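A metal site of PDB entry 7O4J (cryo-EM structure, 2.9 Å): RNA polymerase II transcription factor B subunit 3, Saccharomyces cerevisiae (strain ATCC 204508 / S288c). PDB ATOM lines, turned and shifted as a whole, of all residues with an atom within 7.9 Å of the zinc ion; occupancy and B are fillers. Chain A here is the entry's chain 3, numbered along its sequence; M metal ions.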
ATOM      1  N   ASN A  34     -13.117  28.266 -33.975  1.00  0.00           N
ATOM      2  CA  ASN A  34     -12.896  26.839 -34.173  1.00  0.00           C
ATOM      3  C   ASN A  34     -14.251  26.164 -34.351  1.00  0.00           C
ATOM      4  O   ASN A  34     -15.124  26.305 -33.470  1.00  0.00           O
ATOM      5  CB  ASN A  34     -12.135  26.238 -32.993  1.00  0.00           C
ATOM      6  CG  ASN A  34     -11.864  24.753 -33.177  1.00  0.00           C
ATOM      7  OD1 ASN A  34     -12.243  23.937 -32.339  1.00  0.00           O
ATOM      8  ND2 ASN A  34     -11.221  24.403 -34.276  1.00  0.00           N
ATOM      9  N   GLU A  36     -15.438  23.480 -33.680  1.00  0.00           N
ATOM     10  CA  GLU A  36     -15.870  22.561 -32.617  1.00  0.00           C
ATOM     11  C   GLU A  36     -16.789  23.264 -31.622  1.00  0.00           C
ATOM     12  O   GLU A  36     -17.808  22.688 -31.208  1.00  0.00           O
ATOM     13  CB  GLU A  36     -14.648  21.992 -31.899  1.00  0.00           C
ATOM     14  CG  GLU A  36     -13.787  21.080 -32.756  1.00  0.00           C
ATOM     15  CD  GLU A  36     -14.562  19.885 -33.299  1.00  0.00           C
ATOM     16  OE1 GLU A  36     -15.378  19.317 -32.542  1.00  0.00           O
ATOM     17  OE2 GLU A  36     -14.340  19.522 -34.469  1.00  0.00           O
ATOM     18  N   CYS A  37     -16.452  24.488 -31.227  1.00  0.00           N
ATOM     19  CA  CYS A  37     -17.273  25.226 -30.271  1.00  0.00           C
ATOM     20  C   CYS A  37     -17.550  26.663 -30.682  1.00  0.00           C
ATOM     21  O   CYS A  37     -18.327  27.338 -29.998  1.00  0.00           O
ATOM     22  CB  CYS A  37     -16.617  25.217 -28.879  1.00  0.00           C
ATOM     23  SG  CYS A  37     -14.951  25.899 -28.807  1.00  0.00           S
ATOM     24  N   TYR A  38     -16.965  27.151 -31.775  1.00  0.00           N
ATOM     25  CA  TYR A  38     -17.249  28.477 -32.307  1.00  0.00           C
ATOM     26  C   TYR A  38     -17.094  29.549 -31.234  1.00  0.00           C
ATOM     27  O   TYR A  38     -17.970  30.376 -30.995  1.00  0.00           O
ATOM     28  CB  TYR A  38     -18.659  28.525 -32.910  1.00  0.00           C
ATOM     29  CG  TYR A  38     -18.738  27.883 -34.284  1.00  0.00           C
ATOM     30  CD1 TYR A  38     -18.126  28.468 -35.376  1.00  0.00           C
ATOM     31  CD2 TYR A  38     -19.428  26.689 -34.466  1.00  0.00           C
ATOM     32  CE1 TYR A  38     -18.197  27.887 -36.621  1.00  0.00           C
ATOM     33  CE2 TYR A  38     -19.499  26.108 -35.711  1.00  0.00           C
ATOM     34  CZ  TYR A  38     -18.890  26.709 -36.788  1.00  0.00           C
ATOM     35  OH  TYR A  38     -18.953  26.131 -38.028  1.00  0.00           O
ATOM     36  N   HIS A  39     -15.945  29.517 -30.560  1.00  0.00           N
ATOM     37  CA  HIS A  39     -15.613  30.481 -29.527  1.00  0.00           C
ATOM     38  C   HIS A  39     -14.553  31.442 -30.057  1.00  0.00           C
ATOM     39  O   HIS A  39     -13.483  31.017 -30.508  1.00  0.00           O
ATOM     40  CB  HIS A  39     -15.110  29.772 -28.266  1.00  0.00           C
ATOM     41  CG  HIS A  39     -16.182  29.044 -27.519  1.00  0.00           C
ATOM     42  ND1 HIS A  39     -15.913  27.967 -26.712  1.00  0.00           N
ATOM     43  CD2 HIS A  39     -17.518  29.228 -27.467  1.00  0.00           C
ATOM     44  CE1 HIS A  39     -17.037  27.522 -26.189  1.00  0.00           C
ATOM     45  NE2 HIS A  39     -18.030  28.272 -26.630  1.00  0.00           N
ATOM     46  N   ARG A  40     -14.853  32.737 -29.991  1.00  0.00           N
ATOM     47  CA  ARG A  40     -13.920  33.744 -30.483  1.00  0.00           C
ATOM     48  C   ARG A  40     -12.661  33.772 -29.625  1.00  0.00           C
ATOM     49  O   ARG A  40     -12.729  33.683 -28.393  1.00  0.00           O
ATOM     50  CB  ARG A  40     -14.587  35.114 -30.488  1.00  0.00           C
ATOM     51  CG  ARG A  40     -15.710  35.252 -31.503  1.00  0.00           C
ATOM     52  CD  ARG A  40     -16.321  36.643 -31.473  1.00  0.00           C
ATOM     53  NE  ARG A  40     -15.385  37.663 -31.937  1.00  0.00           N
ATOM     54  CZ  ARG A  40     -14.747  38.527 -31.156  1.00  0.00           C
ATOM     55  NH1 ARG A  40     -14.924  38.526 -29.842  1.00  0.00           N
ATOM     56  NH2 ARG A  40     -13.925  39.421 -31.700  1.00  0.00           N
ATOM     57  N   PHE A  50      -2.003  26.629 -27.635  1.00  0.00           N
ATOM     58  CA  PHE A  50      -2.115  25.458 -28.482  1.00  0.00           C
ATOM     59  C   PHE A  50      -0.856  25.124 -29.273  1.00  0.00           C
ATOM     60  O   PHE A  50      -0.849  24.124 -29.995  1.00  0.00           O
ATOM     61  CB  PHE A  50      -3.270  25.643 -29.475  1.00  0.00           C
ATOM     62  CG  PHE A  50      -4.610  25.865 -28.826  1.00  0.00           C
ATOM     63  CD1 PHE A  50      -5.347  24.796 -28.354  1.00  0.00           C
ATOM     64  CD2 PHE A  50      -5.112  27.147 -28.686  1.00  0.00           C
ATOM     65  CE1 PHE A  50      -6.580  25.003 -27.747  1.00  0.00           C
ATOM     66  CE2 PHE A  50      -6.338  27.354 -28.091  1.00  0.00           C
ATOM     67  CZ  PHE A  50      -7.075  26.285 -27.619  1.00  0.00           C
ATOM     68  N   GLN A  56      -7.549  21.638 -23.967  1.00  0.00           N
ATOM     69  CA  GLN A  56      -8.954  21.975 -23.816  1.00  0.00           C
ATOM     70  C   GLN A  56      -9.169  23.457 -24.097  1.00  0.00           C
ATOM     71  O   GLN A  56      -8.304  24.299 -23.866  1.00  0.00           O
ATOM     72  CB  GLN A  56      -9.437  21.634 -22.402  1.00  0.00           C
ATOM     73  CG  GLN A  56      -8.769  22.434 -21.293  1.00  0.00           C
ATOM     74  CD  GLN A  56      -9.259  22.041 -19.916  1.00  0.00           C
ATOM     75  OE1 GLN A  56      -9.779  20.948 -19.718  1.00  0.00           O
ATOM     76  NE2 GLN A  56      -9.097  22.942 -18.948  1.00  0.00           N
ATOM     77  N   CYS A  57     -10.355  23.764 -24.618  1.00  0.00           N
ATOM     78  CA  CYS A  57     -10.663  25.144 -24.966  1.00  0.00           C
ATOM     79  C   CYS A  57     -10.570  26.021 -23.715  1.00  0.00           C
ATOM     80  O   CYS A  57     -11.067  25.641 -22.651  1.00  0.00           O
ATOM     81  CB  CYS A  57     -12.060  25.238 -25.577  1.00  0.00           C
ATOM     82  SG  CYS A  57     -12.637  26.925 -25.875  1.00  0.00           S
ATOM     83  N   PRO A  58      -9.940  27.199 -23.804  1.00  0.00           N
ATOM     84  CA  PRO A  58      -9.758  28.024 -22.606  1.00  0.00           C
ATOM     85  C   PRO A  58     -10.982  28.869 -22.276  1.00  0.00           C
ATOM     86  O   PRO A  58     -10.850  30.064 -21.991  1.00  0.00           O
ATOM     87  CB  PRO A  58      -8.550  28.891 -22.960  1.00  0.00           C
ATOM     88  CG  PRO A  58      -8.685  29.084 -24.444  1.00  0.00           C
ATOM     89  CD  PRO A  58      -9.367  27.853 -24.995  1.00  0.00           C
ATOM     90  N   TYR A  59     -12.165  28.266 -22.297  1.00  0.00           N
ATOM     91  CA  TYR A  59     -13.402  28.959 -22.016  1.00  0.00           C
ATOM     92  C   TYR A  59     -14.049  28.386 -20.754  1.00  0.00           C
ATOM     93  O   TYR A  59     -13.863  27.227 -20.399  1.00  0.00           O
ATOM     94  CB  TYR A  59     -14.384  28.856 -23.193  1.00  0.00           C
ATOM     95  CG  TYR A  59     -14.346  30.057 -24.109  1.00  0.00           C
ATOM     96  CD1 TYR A  59     -13.153  30.485 -24.673  1.00  0.00           C
ATOM     97  CD2 TYR A  59     -15.506  30.766 -24.396  1.00  0.00           C
ATOM     98  CE1 TYR A  59     -13.127  31.591 -25.513  1.00  0.00           C
ATOM     99  CE2 TYR A  59     -15.482  31.865 -25.229  1.00  0.00           C
ATOM    100  CZ  TYR A  59     -14.287  32.273 -25.784  1.00  0.00           C
ATOM    101  OH  TYR A  59     -14.250  33.368 -26.616  1.00  0.00           O
ATOM    102  N   LYS A  60     -14.829  29.236 -20.088  1.00  0.00           N
ATOM    103  CA  LYS A  60     -15.538  28.862 -18.865  1.00  0.00           C
ATOM    104  C   LYS A  60     -16.782  28.077 -19.257  1.00  0.00           C
ATOM    105  O   LYS A  60     -17.735  28.642 -19.808  1.00  0.00           O
ATOM    106  CB  LYS A  60     -15.901  30.093 -18.047  1.00  0.00           C
ATOM    107  CG  LYS A  60     -14.728  31.043 -17.798  1.00  0.00           C
ATOM    108  CD  LYS A  60     -15.201  32.464 -17.491  1.00  0.00           C
ATOM    109  CE  LYS A  60     -15.796  33.162 -18.717  1.00  0.00           C
ATOM    110  NZ  LYS A  60     -14.922  33.064 -19.923  1.00  0.00           N
ATOM    111  N   GLY A  61     -16.773  26.777 -18.971  1.00  0.00           N
ATOM    112  CA  GLY A  61     -17.876  25.891 -19.309  1.00  0.00           C
ATOM    113  C   GLY A  61     -17.656  25.062 -20.556  1.00  0.00           C
ATOM    114  O   GLY A  61     -18.529  24.239 -20.885  1.00  0.00           O
ATOM    115  N   CYS A  62     -16.532  25.227 -21.248  1.00  0.00           N
ATOM    116  CA  CYS A  62     -16.220  24.468 -22.446  1.00  0.00           C
ATOM    117  C   CYS A  62     -15.025  23.568 -22.162  1.00  0.00           C
ATOM    118  O   CYS A  62     -13.961  24.044 -21.773  1.00  0.00           O
ATOM    119  CB  CYS A  62     -15.910  25.396 -23.617  1.00  0.00           C
ATOM    120  SG  CYS A  62     -15.580  24.550 -25.187  1.00  0.00           S
ATOM    121  N   ASP A  63     -15.220  22.253 -22.352  1.00  0.00           N
ATOM    122  CA  ASP A  63     -14.173  21.265 -22.135  1.00  0.00           C
ATOM    123  C   ASP A  63     -13.902  20.435 -23.384  1.00  0.00           C
ATOM    124  O   ASP A  63     -13.388  19.314 -23.282  1.00  0.00           O
ATOM    125  CB  ASP A  63     -14.540  20.346 -20.958  1.00  0.00           C
ATOM    126  CG  ASP A  63     -14.552  21.081 -19.632  1.00  0.00           C
ATOM    127  OD1 ASP A  63     -14.398  22.317 -19.625  1.00  0.00           O
ATOM    128  OD2 ASP A  63     -14.710  20.411 -18.582  1.00  0.00           O
ATOM    129  N   LYS A  64     -14.230  20.954 -24.554  1.00  0.00           N
ATOM    130  CA  LYS A  64     -14.045  20.239 -25.814  1.00  0.00           C
ATOM    131  C   LYS A  64     -12.664  20.548 -26.370  1.00  0.00           C
ATOM    132  O   LYS A  64     -12.360  21.703 -26.694  1.00  0.00           O
ATOM    133  CB  LYS A  64     -15.132  20.619 -26.814  1.00  0.00           C
ATOM    134  CG  LYS A  64     -16.521  20.111 -26.422  1.00  0.00           C
ATOM    135  CD  LYS A  64     -17.633  20.895 -27.088  1.00  0.00           C
ATOM    136  CE  LYS A  64     -17.738  22.332 -26.568  1.00  0.00           C
ATOM    137  NZ  LYS A  64     -17.612  22.427 -25.082  1.00  0.00           N
ATOM    138  N   ILE A  65     -11.825  19.509 -26.482  1.00  0.00           N
ATOM    139  CA  ILE A  65     -10.454  19.706 -26.936  1.00  0.00           C
ATOM    140  C   ILE A  65     -10.452  20.108 -28.408  1.00  0.00           C
ATOM    141  O   ILE A  65     -11.357  19.768 -29.172  1.00  0.00           O
ATOM    142  CB  ILE A  65      -9.613  18.444 -26.698  1.00  0.00           C
ATOM    143  CG1 ILE A  65      -9.632  18.062 -25.212  1.00  0.00           C
ATOM    144  CG2 ILE A  65      -8.181  18.649 -27.156  1.00  0.00           C
ATOM    145  CD1 ILE A  65      -9.164  16.646 -24.939  1.00  0.00           C
ATOM    146  N   LEU A  66      -9.412  20.840 -28.809  1.00  0.00           N
ATOM    147  CA  LEU A  66      -9.275  21.310 -30.181  1.00  0.00           C
ATOM    148  C   LEU A  66      -7.798  21.501 -30.485  1.00  0.00           C
ATOM    149  O   LEU A  66      -6.965  21.607 -29.584  1.00  0.00           O
ATOM    150  CB  LEU A  66     -10.055  22.607 -30.397  1.00  0.00           C
ATOM    151  CG  LEU A  66      -9.499  23.890 -29.774  1.00  0.00           C
ATOM    152  CD1 LEU A  66     -10.162  25.115 -30.393  1.00  0.00           C
ATOM    153  CD2 LEU A  66      -9.703  23.877 -28.269  1.00  0.00           C
HETATM  154 ZN    ZN M   1     -14.755  26.256 -26.519  1.00  0.00          ZN
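The side-chain sulfur (SG) of Cys 62 sits close to the side-chain amino group (NZ) of Lys 64.
Of the 18 residues printed, 4 come within 4 Å of the zinc ion.
The zinc ion is bound by a ring nitrogen (ND1) of His 39 (2.1 Å), the side-chain sulfur of Cys 57 (2.3 Å), the side-chain sulfur of Cys 62 (2.3 Å) and the side-chain sulfur of Cys 37 (2.3 Å).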
